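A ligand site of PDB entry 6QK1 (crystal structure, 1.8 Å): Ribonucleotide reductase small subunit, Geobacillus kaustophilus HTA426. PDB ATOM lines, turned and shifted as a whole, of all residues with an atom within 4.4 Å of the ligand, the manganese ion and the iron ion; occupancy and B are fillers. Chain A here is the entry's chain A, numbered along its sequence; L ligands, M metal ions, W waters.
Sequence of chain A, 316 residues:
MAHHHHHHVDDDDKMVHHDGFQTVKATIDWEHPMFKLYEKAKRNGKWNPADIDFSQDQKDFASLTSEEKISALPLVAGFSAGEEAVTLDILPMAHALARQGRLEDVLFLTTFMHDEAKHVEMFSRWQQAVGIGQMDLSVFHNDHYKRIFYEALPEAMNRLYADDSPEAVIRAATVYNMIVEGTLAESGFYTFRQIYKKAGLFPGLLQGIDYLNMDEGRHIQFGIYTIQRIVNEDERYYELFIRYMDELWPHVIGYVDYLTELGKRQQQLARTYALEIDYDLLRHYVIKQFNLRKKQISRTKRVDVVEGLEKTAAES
Leu 75 touches the ligand.
Gly 78 touches the ligand.
CE2 of Phe 79 touches C8 of the ligand, 3.6 Å away.
CG2 of Val 86 touches C1 of the ligand (3.7 Å).
Phe 149 touches the ligand.
Val 180 touches the ligand (CG1 to C2, 3.7 Å).
Leu 184 touches the ligand (O to C10, 3.7 Å).
CA of Gly 188 touches C11 of the ligand, at 3.8 Å.
OG1 of Thr 191 touches C13 of the ligand, at 3.4 Å.
Tyr 255 touches the ligand (CE2 to C10, 3.9 Å).
CG1 of Val 256 touches C14 of the ligand, at 3.9 Å.
Leu 282 touches the ligand.
Hydrophobic or aromatic side chains that line the ligand: Leu 75, Phe 79, Val 86, Phe 149, Val 180, Tyr 255, Val 256 and Leu 282.
Of the 25 residues printed, 17 come within 4 Å of the ligand.
The iron ion is bound by an oxygen (O1) of the ligand (1.8 Å), the side-chain carboxylate (OE1) of Glu 116 (2.0 Å), the side-chain carboxylate (OE2) of Glu 181 (2.1 Å), the side-chain carboxylate (OE2) of Glu 216 (2.2 Å), water W1 (2.2 Å) and a ring nitrogen (ND1) of His 219 (2.3 Å).
The iron ion has six donor atoms within binding distance.
O2 of the ligand binds the manganese ion, at 1.7 Å.
ND1 of His 119 is bound to the manganese ion (2.1 Å).
The side-chain carboxylate (OE2) of Glu 83 is bound to the manganese ion (2.1 Å).
The manganese ion is bound by OE2 of Glu 116, at 2.2 Å.
Water W1 binds the manganese ion (2.2 Å).
The manganese ion is bound by water W2 (2.4 Å).
The backbone carbonyl oxygen (O) of Ser 187 sits at hydrogen-bond distance from the side-chain hydroxyl (OG1) of Thr 191 (2.8 Å).
The side-chain hydroxyl of Thr 260 is in hydrogen-bond range of the backbone carbonyl oxygen of Val 256 (3.0 Å).
O of Val 180 lies within hydrogen-bond range of N of Ala 185, at 2.8 Å.
Water W2 bridges OE1 of Glu 83 and OE1 of Glu 216.
Four residues have an atom within 4 Å of the manganese ion: Glu 83, Glu 116, His 119 and Glu 216.
Within 4 Å of the iron ion: Glu 116, Glu 181, Glu 216 and His 219.
Along chain A the residues within 4 Å of the iron ion span positions 116 to 219.
The nearest printed residue that does not touch the iron ion is Phe 112 (4.3 Å).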
ATOM      1  N   LEU A  75     -21.974  22.632 -14.518  1.00  0.00           N
ATOM      2  CA  LEU A  75     -21.456  21.337 -14.969  1.00  0.00           C
ATOM      3  C   LEU A  75     -22.297  20.787 -16.103  1.00  0.00           C
ATOM      4  O   LEU A  75     -21.751  20.241 -17.068  1.00  0.00           O
ATOM      5  CB  LEU A  75     -21.422  20.359 -13.785  1.00  0.00           C
ATOM      6  CG  LEU A  75     -20.772  19.001 -13.980  1.00  0.00           C
ATOM      7  CD1 LEU A  75     -19.315  19.167 -14.426  1.00  0.00           C
ATOM      8  CD2 LEU A  75     -20.853  18.143 -12.672  1.00  0.00           C
ATOM      9  N   GLY A  78     -21.411  22.621 -19.225  1.00  0.00           N
ATOM     10  CA  GLY A  78     -20.188  22.109 -19.826  1.00  0.00           C
ATOM     11  C   GLY A  78     -20.380  20.795 -20.566  1.00  0.00           C
ATOM     12  O   GLY A  78     -19.800  20.579 -21.633  1.00  0.00           O
ATOM     13  N   PHE A  79     -21.178  19.882 -19.996  1.00  0.00           N
ATOM     14  CA  PHE A  79     -21.418  18.605 -20.647  1.00  0.00           C
ATOM     15  C   PHE A  79     -22.291  18.748 -21.899  1.00  0.00           C
ATOM     16  O   PHE A  79     -21.988  18.136 -22.926  1.00  0.00           O
ATOM     17  CB  PHE A  79     -22.041  17.612 -19.678  1.00  0.00           C
ATOM     18  CG  PHE A  79     -21.030  16.700 -19.041  1.00  0.00           C
ATOM     19  CD1 PHE A  79     -20.523  15.631 -19.757  1.00  0.00           C
ATOM     20  CD2 PHE A  79     -20.566  16.924 -17.755  1.00  0.00           C
ATOM     21  CE1 PHE A  79     -19.563  14.763 -19.186  1.00  0.00           C
ATOM     22  CE2 PHE A  79     -19.641  16.057 -17.177  1.00  0.00           C
ATOM     23  CZ  PHE A  79     -19.123  15.001 -17.904  1.00  0.00           C
ATOM     24  N   GLY A  82     -20.310  20.017 -24.597  1.00  0.00           N
ATOM     25  CA  GLY A  82     -19.232  19.108 -24.919  1.00  0.00           C
ATOM     26  C   GLY A  82     -19.692  17.933 -25.739  1.00  0.00           C
ATOM     27  O   GLY A  82     -19.058  17.567 -26.736  1.00  0.00           O
ATOM     28  N   GLU A  83     -20.829  17.316 -25.346  1.00  0.00           N
ATOM     29  CA  GLU A  83     -21.396  16.200 -26.088  1.00  0.00           C
ATOM     30  C   GLU A  83     -21.793  16.640 -27.492  1.00  0.00           C
ATOM     31  O   GLU A  83     -21.649  15.894 -28.461  1.00  0.00           O
ATOM     32  CB  GLU A  83     -22.609  15.604 -25.404  1.00  0.00           C
ATOM     33  CG  GLU A  83     -22.443  15.188 -23.952  1.00  0.00           C
ATOM     34  CD  GLU A  83     -21.452  14.060 -23.738  1.00  0.00           C
ATOM     35  OE1 GLU A  83     -21.054  13.833 -22.566  1.00  0.00           O
ATOM     36  OE2 GLU A  83     -21.077  13.420 -24.751  1.00  0.00           O
ATOM     37  N   VAL A  86     -18.579  17.103 -29.675  1.00  0.00           N
ATOM     38  CA  VAL A  86     -17.917  15.870 -30.121  1.00  0.00           C
ATOM     39  C   VAL A  86     -18.809  15.094 -31.100  1.00  0.00           C
ATOM     40  O   VAL A  86     -18.300  14.431 -32.019  1.00  0.00           O
ATOM     41  CB  VAL A  86     -17.492  15.015 -28.903  1.00  0.00           C
ATOM     42  CG1 VAL A  86     -16.457  15.731 -28.094  1.00  0.00           C
ATOM     43  CG2 VAL A  86     -18.664  14.510 -28.079  1.00  0.00           C
ATOM     44  N   PHE A 112     -19.183   4.922 -31.955  1.00  0.00           N
ATOM     45  CA  PHE A 112     -18.685   6.079 -31.245  1.00  0.00           C
ATOM     46  C   PHE A 112     -19.618   7.269 -31.479  1.00  0.00           C
ATOM     47  O   PHE A 112     -20.067   7.947 -30.523  1.00  0.00           O
ATOM     48  CB  PHE A 112     -17.258   6.354 -31.753  1.00  0.00           C
ATOM     49  CG  PHE A 112     -16.443   7.361 -30.984  1.00  0.00           C
ATOM     50  CD1 PHE A 112     -15.137   7.062 -30.652  1.00  0.00           C
ATOM     51  CD2 PHE A 112     -16.880   8.636 -30.729  1.00  0.00           C
ATOM     52  CE1 PHE A 112     -14.332   7.951 -30.009  1.00  0.00           C
ATOM     53  CE2 PHE A 112     -16.079   9.561 -30.084  1.00  0.00           C
ATOM     54  CZ  PHE A 112     -14.786   9.236 -29.722  1.00  0.00           C
ATOM     55  N   GLU A 116     -22.317   9.323 -28.918  1.00  0.00           N
ATOM     56  CA  GLU A 116     -22.316  10.751 -28.607  1.00  0.00           C
ATOM     57  C   GLU A 116     -23.691  11.353 -28.832  1.00  0.00           C
ATOM     58  O   GLU A 116     -24.118  12.232 -28.085  1.00  0.00           O
ATOM     59  CB  GLU A 116     -21.258  11.501 -29.431  1.00  0.00           C
ATOM     60  CG  GLU A 116     -19.793  10.993 -29.247  1.00  0.00           C
ATOM     61  CD  GLU A 116     -19.280  11.130 -27.804  1.00  0.00           C
ATOM     62  OE1 GLU A 116     -18.105  10.838 -27.582  1.00  0.00           O
ATOM     63  OE2 GLU A 116     -19.991  11.604 -26.894  1.00  0.00           O
ATOM     64  N   HIS A 119     -25.609  10.748 -25.917  1.00  0.00           N
ATOM     65  CA  HIS A 119     -25.166  11.582 -24.797  1.00  0.00           C
ATOM     66  C   HIS A 119     -25.766  12.991 -24.886  1.00  0.00           C
ATOM     67  O   HIS A 119     -26.189  13.569 -23.864  1.00  0.00           O
ATOM     68  CB  HIS A 119     -23.666  11.694 -24.737  1.00  0.00           C
ATOM     69  CG  HIS A 119     -22.976  10.383 -24.561  1.00  0.00           C
ATOM     70  ND1 HIS A 119     -21.598  10.245 -24.544  1.00  0.00           N
ATOM     71  CD2 HIS A 119     -23.494   9.134 -24.425  1.00  0.00           C
ATOM     72  CE1 HIS A 119     -21.313   8.956 -24.370  1.00  0.00           C
ATOM     73  NE2 HIS A 119     -22.434   8.264 -24.331  1.00  0.00           N
ATOM     74  N   PHE A 149     -13.460  23.954 -26.575  1.00  0.00           N
ATOM     75  CA  PHE A 149     -14.605  23.346 -27.235  1.00  0.00           C
ATOM     76  C   PHE A 149     -15.117  24.134 -28.431  1.00  0.00           C
ATOM     77  O   PHE A 149     -15.623  23.522 -29.388  1.00  0.00           O
ATOM     78  CB  PHE A 149     -15.729  23.154 -26.240  1.00  0.00           C
ATOM     79  CG  PHE A 149     -15.498  22.015 -25.290  1.00  0.00           C
ATOM     80  CD1 PHE A 149     -15.799  20.708 -25.660  1.00  0.00           C
ATOM     81  CD2 PHE A 149     -14.946  22.248 -24.037  1.00  0.00           C
ATOM     82  CE1 PHE A 149     -15.565  19.663 -24.778  1.00  0.00           C
ATOM     83  CE2 PHE A 149     -14.730  21.209 -23.164  1.00  0.00           C
ATOM     84  CZ  PHE A 149     -15.038  19.916 -23.543  1.00  0.00           C
ATOM     85  N   VAL A 180     -10.385  16.024 -24.059  1.00  0.00           N
ATOM     86  CA  VAL A 180     -11.826  16.261 -23.860  1.00  0.00           C
ATOM     87  C   VAL A 180     -12.486  15.067 -23.154  1.00  0.00           C
ATOM     88  O   VAL A 180     -13.228  15.237 -22.161  1.00  0.00           O
ATOM     89  CB  VAL A 180     -12.488  16.582 -25.213  1.00  0.00           C
ATOM     90  CG1 VAL A 180     -13.994  16.416 -25.162  1.00  0.00           C
ATOM     91  CG2 VAL A 180     -12.065  17.983 -25.648  1.00  0.00           C
ATOM     92  N   GLU A 181     -12.250  13.845 -23.652  1.00  0.00           N
ATOM     93  CA  GLU A 181     -12.868  12.636 -23.101  1.00  0.00           C
ATOM     94  C   GLU A 181     -12.063  12.126 -21.925  1.00  0.00           C
ATOM     95  O   GLU A 181     -12.592  11.918 -20.822  1.00  0.00           O
ATOM     96  CB  GLU A 181     -13.007  11.532 -24.170  1.00  0.00           C
ATOM     97  CG  GLU A 181     -13.887  11.906 -25.374  1.00  0.00           C
ATOM     98  CD  GLU A 181     -14.005  10.799 -26.392  1.00  0.00           C
ATOM     99  OE1 GLU A 181     -12.976  10.161 -26.712  1.00  0.00           O
ATOM    100  OE2 GLU A 181     -15.134  10.510 -26.833  1.00  0.00           O
ATOM    101  N   LEU A 184     -11.276  15.660 -19.246  1.00  0.00           N
ATOM    102  CA  LEU A 184     -12.380  16.486 -18.761  1.00  0.00           C
ATOM    103  C   LEU A 184     -13.620  15.645 -18.504  1.00  0.00           C
ATOM    104  O   LEU A 184     -14.224  15.742 -17.418  1.00  0.00           O
ATOM    105  CB  LEU A 184     -12.679  17.621 -19.757  1.00  0.00           C
ATOM    106  CG  LEU A 184     -11.699  18.768 -19.756  1.00  0.00           C
ATOM    107  CD1 LEU A 184     -11.924  19.674 -20.982  1.00  0.00           C
ATOM    108  CD2 LEU A 184     -11.750  19.610 -18.487  1.00  0.00           C
ATOM    109  N   ALA A 185     -14.044  14.838 -19.488  1.00  0.00           N
ATOM    110  CA  ALA A 185     -15.248  14.032 -19.299  1.00  0.00           C
ATOM    111  C   ALA A 185     -15.130  13.113 -18.077  1.00  0.00           C
ATOM    112  O   ALA A 185     -16.050  13.009 -17.240  1.00  0.00           O
ATOM    113  CB  ALA A 185     -15.544  13.192 -20.541  1.00  0.00           C
ATOM    114  N   SER A 187     -13.333  13.334 -15.460  1.00  0.00           N
ATOM    115  CA  SER A 187     -13.359  14.095 -14.227  1.00  0.00           C
ATOM    116  C   SER A 187     -14.762  14.623 -13.945  1.00  0.00           C
ATOM    117  O   SER A 187     -15.167  14.701 -12.790  1.00  0.00           O
ATOM    118  CB  SER A 187     -12.360  15.259 -14.260  1.00  0.00           C
ATOM    119  OG  SER A 187     -11.031  14.851 -14.490  1.00  0.00           O
ATOM    120  N   GLY A 188     -15.524  14.989 -14.983  1.00  0.00           N
ATOM    121  CA  GLY A 188     -16.900  15.420 -14.751  1.00  0.00           C
ATOM    122  C   GLY A 188     -17.791  14.292 -14.299  1.00  0.00           C
ATOM    123  O   GLY A 188     -18.699  14.498 -13.483  1.00  0.00           O
ATOM    124  N   THR A 191     -16.966  14.040 -10.695  1.00  0.00           N
ATOM    125  CA  THR A 191     -17.543  15.170  -9.956  1.00  0.00           C
ATOM    126  C   THR A 191     -19.046  14.965  -9.719  1.00  0.00           C
ATOM    127  O   THR A 191     -19.541  15.225  -8.613  1.00  0.00           O
ATOM    128  CB  THR A 191     -17.254  16.465 -10.720  1.00  0.00           C
ATOM    129  OG1 THR A 191     -15.849  16.648 -10.841  1.00  0.00           O
ATOM    130  CG2 THR A 191     -17.848  17.681 -10.055  1.00  0.00           C
ATOM    131  N   GLU A 216     -17.804   5.914 -22.684  1.00  0.00           N
ATOM    132  CA  GLU A 216     -16.590   6.713 -22.782  1.00  0.00           C
ATOM    133  C   GLU A 216     -15.347   5.843 -22.718  1.00  0.00           C
ATOM    134  O   GLU A 216     -14.335   6.150 -23.348  1.00  0.00           O
ATOM    135  CB  GLU A 216     -16.542   7.705 -21.642  1.00  0.00           C
ATOM    136  CG  GLU A 216     -15.695   8.849 -21.920  1.00  0.00           C
ATOM    137  CD  GLU A 216     -16.422   9.731 -22.902  1.00  0.00           C
ATOM    138  OE1 GLU A 216     -17.437  10.328 -22.493  1.00  0.00           O
ATOM    139  OE2 GLU A 216     -16.026   9.729 -24.083  1.00  0.00           O
ATOM    140  N   HIS A 219     -14.419   4.947 -26.172  1.00  0.00           N
ATOM    141  CA  HIS A 219     -13.893   6.106 -26.897  1.00  0.00           C
ATOM    142  C   HIS A 219     -12.420   6.358 -26.561  1.00  0.00           C
ATOM    143  O   HIS A 219     -11.603   6.595 -27.445  1.00  0.00           O
ATOM    144  CB  HIS A 219     -14.741   7.344 -26.575  1.00  0.00           C
ATOM    145  CG  HIS A 219     -16.198   7.163 -26.832  1.00  0.00           C
ATOM    146  ND1 HIS A 219     -17.128   8.170 -26.654  1.00  0.00           N
ATOM    147  CD2 HIS A 219     -16.899   6.080 -27.253  1.00  0.00           C
ATOM    148  CE1 HIS A 219     -18.334   7.699 -26.932  1.00  0.00           C
ATOM    149  NE2 HIS A 219     -18.212   6.440 -27.310  1.00  0.00           N
ATOM    150  N   TYR A 255     -10.424  26.065 -16.833  1.00  0.00           N
ATOM    151  CA  TYR A 255     -11.842  25.810 -16.737  1.00  0.00           C
ATOM    152  C   TYR A 255     -12.190  25.166 -15.386  1.00  0.00           C
ATOM    153  O   TYR A 255     -13.210  25.505 -14.766  1.00  0.00           O
ATOM    154  CB  TYR A 255     -12.283  24.937 -17.899  1.00  0.00           C
ATOM    155  CG  TYR A 255     -13.732  24.514 -17.845  1.00  0.00           C
ATOM    156  CD1 TYR A 255     -14.768  25.456 -17.783  1.00  0.00           C
ATOM    157  CD2 TYR A 255     -14.087  23.163 -17.855  1.00  0.00           C
ATOM    158  CE1 TYR A 255     -16.108  25.044 -17.741  1.00  0.00           C
ATOM    159  CE2 TYR A 255     -15.427  22.752 -17.814  1.00  0.00           C
ATOM    160  CZ  TYR A 255     -16.431  23.698 -17.771  1.00  0.00           C
ATOM    161  OH  TYR A 255     -17.753  23.224 -17.715  1.00  0.00           O
ATOM    162  N   VAL A 256     -11.365  24.227 -14.930  1.00  0.00           N
ATOM    163  CA  VAL A 256     -11.569  23.612 -13.630  1.00  0.00           C
ATOM    164  C   VAL A 256     -11.574  24.678 -12.540  1.00  0.00           C
ATOM    165  O   VAL A 256     -12.441  24.670 -11.650  1.00  0.00           O
ATOM    166  CB  VAL A 256     -10.496  22.530 -13.360  1.00  0.00           C
ATOM    167  CG1 VAL A 256     -10.600  22.032 -11.926  1.00  0.00           C
ATOM    168  CG2 VAL A 256     -10.654  21.371 -14.333  1.00  0.00           C
ATOM    169  N   LEU A 259     -14.889  26.685 -12.628  1.00  0.00           N
ATOM    170  CA  LEU A 259     -15.991  25.924 -12.016  1.00  0.00           C
ATOM    171  C   LEU A 259     -15.833  25.812 -10.506  1.00  0.00           C
ATOM    172  O   LEU A 259     -16.827  25.827  -9.774  1.00  0.00           O
ATOM    173  CB  LEU A 259     -16.071  24.529 -12.606  1.00  0.00           C
ATOM    174  CG  LEU A 259     -16.541  24.385 -14.036  1.00  0.00           C
ATOM    175  CD1 LEU A 259     -16.390  22.891 -14.340  1.00  0.00           C
ATOM    176  CD2 LEU A 259     -17.977  24.885 -14.220  1.00  0.00           C
ATOM    177  N   THR A 260     -14.598  25.640 -10.039  1.00  0.00           N
ATOM    178  CA  THR A 260     -14.321  25.604  -8.599  1.00  0.00           C
ATOM    179  C   THR A 260     -14.722  26.910  -7.924  1.00  0.00           C
ATOM    180  O   THR A 260     -15.404  26.911  -6.894  1.00  0.00           O
ATOM    181  CB  THR A 260     -12.848  25.305  -8.381  1.00  0.00           C
ATOM    182  OG1 THR A 260     -12.598  23.928  -8.709  1.00  0.00           O
ATOM    183  CG2 THR A 260     -12.425  25.572  -6.941  1.00  0.00           C
ATOM    184  N   LEU A 282     -11.271  17.195  -6.124  1.00  0.00           N
ATOM    185  CA  LEU A 282     -11.692  17.245  -7.517  1.00  0.00           C
ATOM    186  C   LEU A 282     -10.567  17.732  -8.405  1.00  0.00           C
ATOM    187  O   LEU A 282     -10.266  17.126  -9.444  1.00  0.00           O
ATOM    188  CB  LEU A 282     -12.918  18.143  -7.658  1.00  0.00           C
ATOM    189  CG  LEU A 282     -14.236  17.723  -7.008  1.00  0.00           C
ATOM    190  CD1 LEU A 282     -15.365  18.706  -7.370  1.00  0.00           C
ATOM    191  CD2 LEU A 282     -14.625  16.279  -7.350  1.00  0.00           C
ATOM    192  N   VAL A 286      -8.451  15.623 -11.512  1.00  0.00           N
ATOM    193  CA  VAL A 286      -8.197  16.133 -12.871  1.00  0.00           C
ATOM    194  C   VAL A 286      -6.730  15.989 -13.203  1.00  0.00           C
ATOM    195  O   VAL A 286      -6.366  15.479 -14.271  1.00  0.00           O
ATOM    196  CB  VAL A 286      -8.636  17.607 -12.988  1.00  0.00           C
ATOM    197  CG1 VAL A 286      -8.174  18.212 -14.351  1.00  0.00           C
ATOM    198  CG2 VAL A 286     -10.099  17.739 -12.859  1.00  0.00           C
HETATM  199  C1  LIG L   1     -17.598  12.977 -24.844  1.00  0.00           C
HETATM  200  O1  LIG L   1     -16.841  12.105 -25.514  1.00  0.00           O
HETATM  201  O2  LIG L   1     -18.804  12.818 -24.499  1.00  0.00           O
HETATM  202  C2  LIG L   1     -16.936  14.364 -24.376  1.00  0.00           C
HETATM  203  C3  LIG L   1     -17.727  15.245 -23.371  1.00  0.00           C
HETATM  204  C4  LIG L   1     -16.972  16.402 -22.767  1.00  0.00           C
HETATM  205  C5  LIG L   1     -17.568  16.969 -21.436  1.00  0.00           C
HETATM  206  C6  LIG L   1     -17.069  18.306 -21.084  1.00  0.00           C
HETATM  207  C7  LIG L   1     -17.588  18.889 -19.719  1.00  0.00           C
HETATM  208  C8  LIG L   1     -17.049  18.156 -18.541  1.00  0.00           C
HETATM  209  C9  LIG L   1     -17.029  18.965 -17.229  1.00  0.00           C
HETATM  210  C10 LIG L   1     -15.612  19.080 -16.625  1.00  0.00           C
HETATM  211  C11 LIG L   1     -15.609  18.997 -15.131  1.00  0.00           C
HETATM  212  C12 LIG L   1     -14.204  18.871 -14.512  1.00  0.00           C
HETATM  213  C13 LIG L   1     -14.298  18.809 -12.976  1.00  0.00           C
HETATM  214  C14 LIG L   1     -14.054  20.149 -12.248  1.00  0.00           C
HETATM  215  C15 LIG L   1     -14.415  20.160 -10.745  1.00  0.00           C
HETATM  216  C16 LIG L   1     -15.355  21.310 -10.324  1.00  0.00           C
HETATM  217 MN    MN M   1     -19.982  11.604 -24.737  1.00  0.00          MN
HETATM  218 FE    FE M   2     -16.990  10.386 -25.939  1.00  0.00          FE
HETATM  219  O   HOH W   1     -18.649   9.831 -24.584  1.00  0.00           O
HETATM  220  O   HOH W   2     -19.735  11.709 -22.388  1.00  0.00           O
